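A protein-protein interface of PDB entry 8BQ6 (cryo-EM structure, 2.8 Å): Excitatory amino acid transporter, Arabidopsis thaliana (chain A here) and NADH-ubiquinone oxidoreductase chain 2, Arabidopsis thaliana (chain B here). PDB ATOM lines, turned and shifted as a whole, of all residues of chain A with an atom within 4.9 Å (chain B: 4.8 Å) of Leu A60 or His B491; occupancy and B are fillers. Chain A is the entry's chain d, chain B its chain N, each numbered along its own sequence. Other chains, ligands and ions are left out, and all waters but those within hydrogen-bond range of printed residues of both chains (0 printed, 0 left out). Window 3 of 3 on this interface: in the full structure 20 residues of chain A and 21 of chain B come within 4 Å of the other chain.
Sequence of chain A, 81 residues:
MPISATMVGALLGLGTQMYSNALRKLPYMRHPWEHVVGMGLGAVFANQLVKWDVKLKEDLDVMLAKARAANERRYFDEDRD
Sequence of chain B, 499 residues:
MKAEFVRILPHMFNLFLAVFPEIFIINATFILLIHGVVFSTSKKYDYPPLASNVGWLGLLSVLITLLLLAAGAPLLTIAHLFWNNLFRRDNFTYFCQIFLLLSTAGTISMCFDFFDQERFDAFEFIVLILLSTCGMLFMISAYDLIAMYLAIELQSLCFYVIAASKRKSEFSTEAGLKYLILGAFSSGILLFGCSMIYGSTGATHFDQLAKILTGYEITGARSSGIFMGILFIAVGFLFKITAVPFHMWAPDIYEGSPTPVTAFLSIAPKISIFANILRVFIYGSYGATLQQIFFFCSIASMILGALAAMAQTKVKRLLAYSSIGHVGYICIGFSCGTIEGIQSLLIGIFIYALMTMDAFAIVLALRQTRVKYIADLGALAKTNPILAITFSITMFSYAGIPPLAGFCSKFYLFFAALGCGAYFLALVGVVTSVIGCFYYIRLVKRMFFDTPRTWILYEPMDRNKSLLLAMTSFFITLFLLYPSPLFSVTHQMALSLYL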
ATOM      1  N   LEU A  56      22.829  -8.010  -2.120  1.00  0.00           N
ATOM      2  CA  LEU A  56      23.098  -6.733  -2.835  1.00  0.00           C
ATOM      3  C   LEU A  56      22.347  -5.587  -2.160  1.00  0.00           C
ATOM      4  O   LEU A  56      22.972  -4.534  -1.947  1.00  0.00           O
ATOM      5  CB  LEU A  56      22.626  -6.883  -4.281  1.00  0.00           C
ATOM      6  CG  LEU A  56      23.688  -7.303  -5.290  1.00  0.00           C
ATOM      7  CD1 LEU A  56      23.083  -7.350  -6.680  1.00  0.00           C
ATOM      8  CD2 LEU A  56      24.876  -6.356  -5.253  1.00  0.00           C
ATOM      9  N   LYS A  57      21.059  -5.783  -1.860  1.00  0.00           N
ATOM     10  CA  LYS A  57      20.228  -4.722  -1.227  1.00  0.00           C
ATOM     11  C   LYS A  57      20.876  -4.269   0.086  1.00  0.00           C
ATOM     12  O   LYS A  57      21.023  -3.051   0.260  1.00  0.00           O
ATOM     13  CB  LYS A  57      18.800  -5.224  -1.001  1.00  0.00           C
ATOM     14  CG  LYS A  57      18.002  -5.486  -2.271  1.00  0.00           C
ATOM     15  CD  LYS A  57      16.605  -6.004  -2.009  1.00  0.00           C
ATOM     16  CE  LYS A  57      15.817  -6.235  -3.280  1.00  0.00           C
ATOM     17  NZ  LYS A  57      14.461  -6.764  -3.000  1.00  0.00           N
ATOM     18  N   GLU A  58      21.253  -5.211   0.960  1.00  0.00           N
ATOM     19  CA  GLU A  58      21.928  -4.867   2.243  1.00  0.00           C
ATOM     20  C   GLU A  58      23.162  -4.001   1.967  1.00  0.00           C
ATOM     21  O   GLU A  58      23.270  -2.930   2.592  1.00  0.00           O
ATOM     22  CB  GLU A  58      22.366  -6.121   2.996  1.00  0.00           C
ATOM     23  CG  GLU A  58      21.263  -7.141   3.199  1.00  0.00           C
ATOM     24  CD  GLU A  58      21.760  -8.563   3.394  1.00  0.00           C
ATOM     25  OE1 GLU A  58      21.024  -9.499   3.029  1.00  0.00           O
ATOM     26  OE2 GLU A  58      22.882  -8.733   3.912  1.00  0.00           O
ATOM     27  N   ASP A  59      24.052  -4.453   1.077  1.00  0.00           N
ATOM     28  CA  ASP A  59      25.299  -3.702   0.763  1.00  0.00           C
ATOM     29  C   ASP A  59      24.946  -2.293   0.279  1.00  0.00           C
ATOM     30  O   ASP A  59      25.586  -1.337   0.752  1.00  0.00           O
ATOM     31  CB  ASP A  59      26.155  -4.435  -0.272  1.00  0.00           C
ATOM     32  CG  ASP A  59      26.294  -5.925  -0.016  1.00  0.00           C
ATOM     33  OD1 ASP A  59      26.376  -6.313   1.167  1.00  0.00           O
ATOM     34  OD2 ASP A  59      26.316  -6.687  -1.002  1.00  0.00           O
ATOM     35  N   LEU A  60      23.969  -2.179  -0.627  1.00  0.00           N
ATOM     36  CA  LEU A  60      23.545  -0.857  -1.159  1.00  0.00           C
ATOM     37  C   LEU A  60      23.055   0.034  -0.012  1.00  0.00           C
ATOM     38  O   LEU A  60      23.424   1.214  -0.007  1.00  0.00           O
ATOM     39  CB  LEU A  60      22.438  -1.064  -2.196  1.00  0.00           C
ATOM     40  CG  LEU A  60      22.140   0.155  -3.065  1.00  0.00           C
ATOM     41  CD1 LEU A  60      23.425   0.721  -3.643  1.00  0.00           C
ATOM     42  CD2 LEU A  60      21.159  -0.194  -4.171  1.00  0.00           C
ATOM     43  N   ASP A  61      22.249  -0.510   0.905  1.00  0.00           N
ATOM     44  CA  ASP A  61      21.725   0.275   2.056  1.00  0.00           C
ATOM     45  C   ASP A  61      22.896   0.845   2.864  1.00  0.00           C
ATOM     46  O   ASP A  61      22.840   2.040   3.189  1.00  0.00           O
ATOM     47  CB  ASP A  61      20.788  -0.558   2.935  1.00  0.00           C
ATOM     48  CG  ASP A  61      19.531  -1.021   2.217  1.00  0.00           C
ATOM     49  OD1 ASP A  61      19.062  -0.291   1.321  1.00  0.00           O
ATOM     50  OD2 ASP A  61      19.037  -2.114   2.558  1.00  0.00           O
ATOM     51  N   VAL A  62      23.902   0.019   3.175  1.00  0.00           N
ATOM     52  CA  VAL A  62      25.109   0.491   3.919  1.00  0.00           C
ATOM     53  C   VAL A  62      25.777   1.618   3.121  1.00  0.00           C
ATOM     54  O   VAL A  62      26.077   2.666   3.723  1.00  0.00           O
ATOM     55  CB  VAL A  62      26.088  -0.669   4.190  1.00  0.00           C
ATOM     56  CG1 VAL A  62      27.344  -0.208   4.914  1.00  0.00           C
ATOM     57  CG2 VAL A  62      25.422  -1.802   4.954  1.00  0.00           C
ATOM     58  N   MET A  63      25.991   1.409   1.819  1.00  0.00           N
ATOM     59  CA  MET A  63      26.639   2.435   0.958  1.00  0.00           C
ATOM     60  C   MET A  63      25.800   3.718   0.947  1.00  0.00           C
ATOM     61  O   MET A  63      26.401   4.804   1.034  1.00  0.00           O
ATOM     62  CB  MET A  63      26.796   1.918  -0.474  1.00  0.00           C
ATOM     63  CG  MET A  63      27.793   0.786  -0.596  1.00  0.00           C
ATOM     64  SD  MET A  63      27.892   0.141  -2.280  1.00  0.00           S
ATOM     65  CE  MET A  63      28.745   1.490  -3.096  1.00  0.00           C
ATOM     66  N   LEU A  64      24.470   3.601   0.841  1.00  0.00           N
ATOM     67  CA  LEU A  64      23.613   4.778   0.788  1.00  0.00           C
ATOM     68  C   LEU A  64      23.604   5.505   2.127  1.00  0.00           C
ATOM     69  O   LEU A  64      23.554   6.741   2.172  1.00  0.00           O
ATOM     70  CB  LEU A  64      22.198   4.384   0.375  1.00  0.00           C
ATOM     71  CG  LEU A  64      21.837   4.738  -1.064  1.00  0.00           C
ATOM     72  CD1 LEU A  64      20.545   4.058  -1.470  1.00  0.00           C
ATOM     73  CD2 LEU A  64      21.714   6.238  -1.183  1.00  0.00           C
ATOM     74  N   ALA A  65      23.675   4.754   3.229  1.00  0.00           N
ATOM     75  CA  ALA A  65      23.781   5.372   4.545  1.00  0.00           C
ATOM     76  C   ALA A  65      25.036   6.228   4.639  1.00  0.00           C
ATOM     77  O   ALA A  65      24.990   7.377   5.101  1.00  0.00           O
ATOM     78  CB  ALA A  65      23.784   4.292   5.627  1.00  0.00           C
ATOM     79  N   ILE B 339      24.909  10.476 -10.328  1.00  0.00           N
ATOM     80  CA  ILE B 339      24.893   9.078  -9.899  1.00  0.00           C
ATOM     81  C   ILE B 339      24.043   8.245 -10.850  1.00  0.00           C
ATOM     82  O   ILE B 339      24.423   7.137 -11.253  1.00  0.00           O
ATOM     83  CB  ILE B 339      24.381   8.965  -8.452  1.00  0.00           C
ATOM     84  CG1 ILE B 339      25.458   9.367  -7.454  1.00  0.00           C
ATOM     85  CG2 ILE B 339      23.996   7.540  -8.145  1.00  0.00           C
ATOM     86  CD1 ILE B 339      26.686   8.525  -7.544  1.00  0.00           C
ATOM     87  N   GLN B 343      25.130   5.048 -13.203  1.00  0.00           N
ATOM     88  CA  GLN B 343      24.373   3.805 -13.121  1.00  0.00           C
ATOM     89  C   GLN B 343      23.831   3.407 -14.483  1.00  0.00           C
ATOM     90  O   GLN B 343      23.923   2.240 -14.884  1.00  0.00           O
ATOM     91  CB  GLN B 343      23.219   3.933 -12.132  1.00  0.00           C
ATOM     92  CG  GLN B 343      22.611   2.591 -11.783  1.00  0.00           C
ATOM     93  CD  GLN B 343      21.343   2.710 -10.973  1.00  0.00           C
ATOM     94  OE1 GLN B 343      20.781   3.793 -10.836  1.00  0.00           O
ATOM     95  NE2 GLN B 343      20.885   1.591 -10.429  1.00  0.00           N
ATOM     96  N   LEU B 486      20.655  -6.216 -11.279  1.00  0.00           N
ATOM     97  CA  LEU B 486      21.500  -5.324 -12.067  1.00  0.00           C
ATOM     98  C   LEU B 486      21.390  -3.887 -11.573  1.00  0.00           C
ATOM     99  O   LEU B 486      22.397  -3.176 -11.486  1.00  0.00           O
ATOM    100  CB  LEU B 486      21.135  -5.404 -13.551  1.00  0.00           C
ATOM    101  CG  LEU B 486      22.069  -4.671 -14.524  1.00  0.00           C
ATOM    102  CD1 LEU B 486      23.524  -5.135 -14.398  1.00  0.00           C
ATOM    103  CD2 LEU B 486      21.576  -4.766 -15.960  1.00  0.00           C
ATOM    104  N   PHE B 487      20.177  -3.445 -11.243  1.00  0.00           N
ATOM    105  CA  PHE B 487      19.991  -2.083 -10.748  1.00  0.00           C
ATOM    106  C   PHE B 487      20.746  -1.873  -9.449  1.00  0.00           C
ATOM    107  O   PHE B 487      21.463  -0.877  -9.279  1.00  0.00           O
ATOM    108  CB  PHE B 487      18.507  -1.800 -10.551  1.00  0.00           C
ATOM    109  CG  PHE B 487      17.734  -1.760 -11.819  1.00  0.00           C
ATOM    110  CD1 PHE B 487      18.387  -1.720 -13.037  1.00  0.00           C
ATOM    111  CD2 PHE B 487      16.358  -1.783 -11.803  1.00  0.00           C
ATOM    112  CE1 PHE B 487      17.679  -1.684 -14.210  1.00  0.00           C
ATOM    113  CE2 PHE B 487      15.647  -1.751 -12.974  1.00  0.00           C
ATOM    114  CZ  PHE B 487      16.309  -1.701 -14.179  1.00  0.00           C
ATOM    115  N   SER B 488      20.612  -2.824  -8.525  1.00  0.00           N
ATOM    116  CA  SER B 488      21.308  -2.718  -7.252  1.00  0.00           C
ATOM    117  C   SER B 488      22.821  -2.729  -7.441  1.00  0.00           C
ATOM    118  O   SER B 488      23.528  -1.913  -6.839  1.00  0.00           O
ATOM    119  CB  SER B 488      20.875  -3.850  -6.327  1.00  0.00           C
ATOM    120  OG  SER B 488      21.628  -3.831  -5.130  1.00  0.00           O
ATOM    121  N   VAL B 489      23.337  -3.631  -8.280  1.00  0.00           N
ATOM    122  CA  VAL B 489      24.786  -3.755  -8.414  1.00  0.00           C
ATOM    123  C   VAL B 489      25.371  -2.537  -9.116  1.00  0.00           C
ATOM    124  O   VAL B 489      26.459  -2.067  -8.763  1.00  0.00           O
ATOM    125  CB  VAL B 489      25.169  -5.071  -9.119  1.00  0.00           C
ATOM    126  CG1 VAL B 489      24.848  -5.033 -10.599  1.00  0.00           C
ATOM    127  CG2 VAL B 489      26.640  -5.341  -8.921  1.00  0.00           C
ATOM    128  N   THR B 490      24.664  -1.989 -10.106  1.00  0.00           N
ATOM    129  CA  THR B 490      25.182  -0.806 -10.778  1.00  0.00           C
ATOM    130  C   THR B 490      25.117   0.413  -9.868  1.00  0.00           C
ATOM    131  O   THR B 490      26.018   1.258  -9.898  1.00  0.00           O
ATOM    132  CB  THR B 490      24.422  -0.561 -12.078  1.00  0.00           C
ATOM    133  OG1 THR B 490      23.023  -0.756 -11.856  1.00  0.00           O
ATOM    134  CG2 THR B 490      24.893  -1.537 -13.149  1.00  0.00           C
ATOM    135  N   HIS B 491      24.067   0.524  -9.046  1.00  0.00           N
ATOM    136  CA  HIS B 491      24.032   1.587  -8.045  1.00  0.00           C
ATOM    137  C   HIS B 491      25.201   1.457  -7.077  1.00  0.00           C
ATOM    138  O   HIS B 491      25.832   2.454  -6.704  1.00  0.00           O
ATOM    139  CB  HIS B 491      22.704   1.543  -7.292  1.00  0.00           C
ATOM    140  CG  HIS B 491      22.363   2.815  -6.579  1.00  0.00           C
ATOM    141  ND1 HIS B 491      21.093   3.349  -6.591  1.00  0.00           N
ATOM    142  CD2 HIS B 491      23.110   3.639  -5.809  1.00  0.00           C
ATOM    143  CE1 HIS B 491      21.078   4.460  -5.876  1.00  0.00           C
ATOM    144  NE2 HIS B 491      22.289   4.656  -5.387  1.00  0.00           N
ATOM    145  N   GLN B 492      25.503   0.214  -6.695  1.00  0.00           N
ATOM    146  CA  GLN B 492      26.665  -0.044  -5.808  1.00  0.00           C
ATOM    147  C   GLN B 492      27.932   0.465  -6.504  1.00  0.00           C
ATOM    148  O   GLN B 492      28.685   1.199  -5.852  1.00  0.00           O
ATOM    149  CB  GLN B 492      26.722  -1.536  -5.474  1.00  0.00           C
ATOM    150  CG  GLN B 492      28.018  -1.997  -4.826  1.00  0.00           C
ATOM    151  CD  GLN B 492      27.815  -3.204  -3.943  1.00  0.00           C
ATOM    152  OE1 GLN B 492      26.692  -3.616  -3.661  1.00  0.00           O
ATOM    153  NE2 GLN B 492      28.915  -3.783  -3.490  1.00  0.00           N
ATOM    154  N   MET B 493      28.132   0.127  -7.786  1.00  0.00           N
ATOM    155  CA  MET B 493      29.354   0.531  -8.482  1.00  0.00           C
ATOM    156  C   MET B 493      29.449   2.049  -8.608  1.00  0.00           C
ATOM    157  O   MET B 493      30.511   2.644  -8.356  1.00  0.00           O
ATOM    158  CB  MET B 493      29.418  -0.135  -9.856  1.00  0.00           C
ATOM    159  CG  MET B 493      29.294  -1.648  -9.815  1.00  0.00           C
ATOM    160  SD  MET B 493      29.036  -2.375 -11.441  1.00  0.00           S
ATOM    161  CE  MET B 493      30.552  -1.907 -12.263  1.00  0.00           C
ATOM    162  N   ALA B 494      28.338   2.696  -8.970  1.00  0.00           N
ATOM    163  CA  ALA B 494      28.317   4.148  -9.086  1.00  0.00           C
ATOM    164  C   ALA B 494      28.672   4.807  -7.760  1.00  0.00           C
ATOM    165  O   ALA B 494      29.406   5.803  -7.726  1.00  0.00           O
ATOM    166  CB  ALA B 494      26.946   4.616  -9.574  1.00  0.00           C
ATOM    167  N   LEU B 495      28.163   4.266  -6.649  1.00  0.00           N
ATOM    168  CA  LEU B 495      28.527   4.819  -5.347  1.00  0.00           C
ATOM    169  C   LEU B 495      29.984   4.539  -5.010  1.00  0.00           C
ATOM    170  O   LEU B 495      30.683   5.408  -4.478  1.00  0.00           O
ATOM    171  CB  LEU B 495      27.615   4.263  -4.254  1.00  0.00           C
ATOM    172  CG  LEU B 495      26.371   5.076  -3.898  1.00  0.00           C
ATOM    173  CD1 LEU B 495      25.734   5.674  -5.132  1.00  0.00           C
ATOM    174  CD2 LEU B 495      25.377   4.210  -3.156  1.00  0.00           C
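Of the 12 printed residues of chain B, 5 touch a printed residue of chain A.
Hydrophobic or aromatic side chains of chain B that line the printed part of chain A: Val B489, His B491 and Leu B495.
Along chain B the printed residues that touch a printed residue of chain A span positions 488 to 495.
Printed residues of chain A within 4 Å of Leu B495: Met A63.
Of the printed residues of chain A, Gln B492 touches Leu A56, Asp A59, Leu A60 and Met A63.
Among the printed residues, pairs that only touch across the chains: Met A63 with Gln B492 (2.8 Å), Met A63 with Leu B495 (3.2 Å), Leu A56 with Ser B488 (3.3 Å), Asp A59 with Gln B492 (3.5 Å), Leu A60 with His B491 (3.6 Å), Leu A56 with Gln B492 (3.7 Å), Leu A60 with Gln B492 (3.7 Å), Leu A60 with Ser B488 (3.8 Å), Lys A57 with Ser B488 (3.9 Å) and Leu A56 with Val B489 (3.9 Å).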
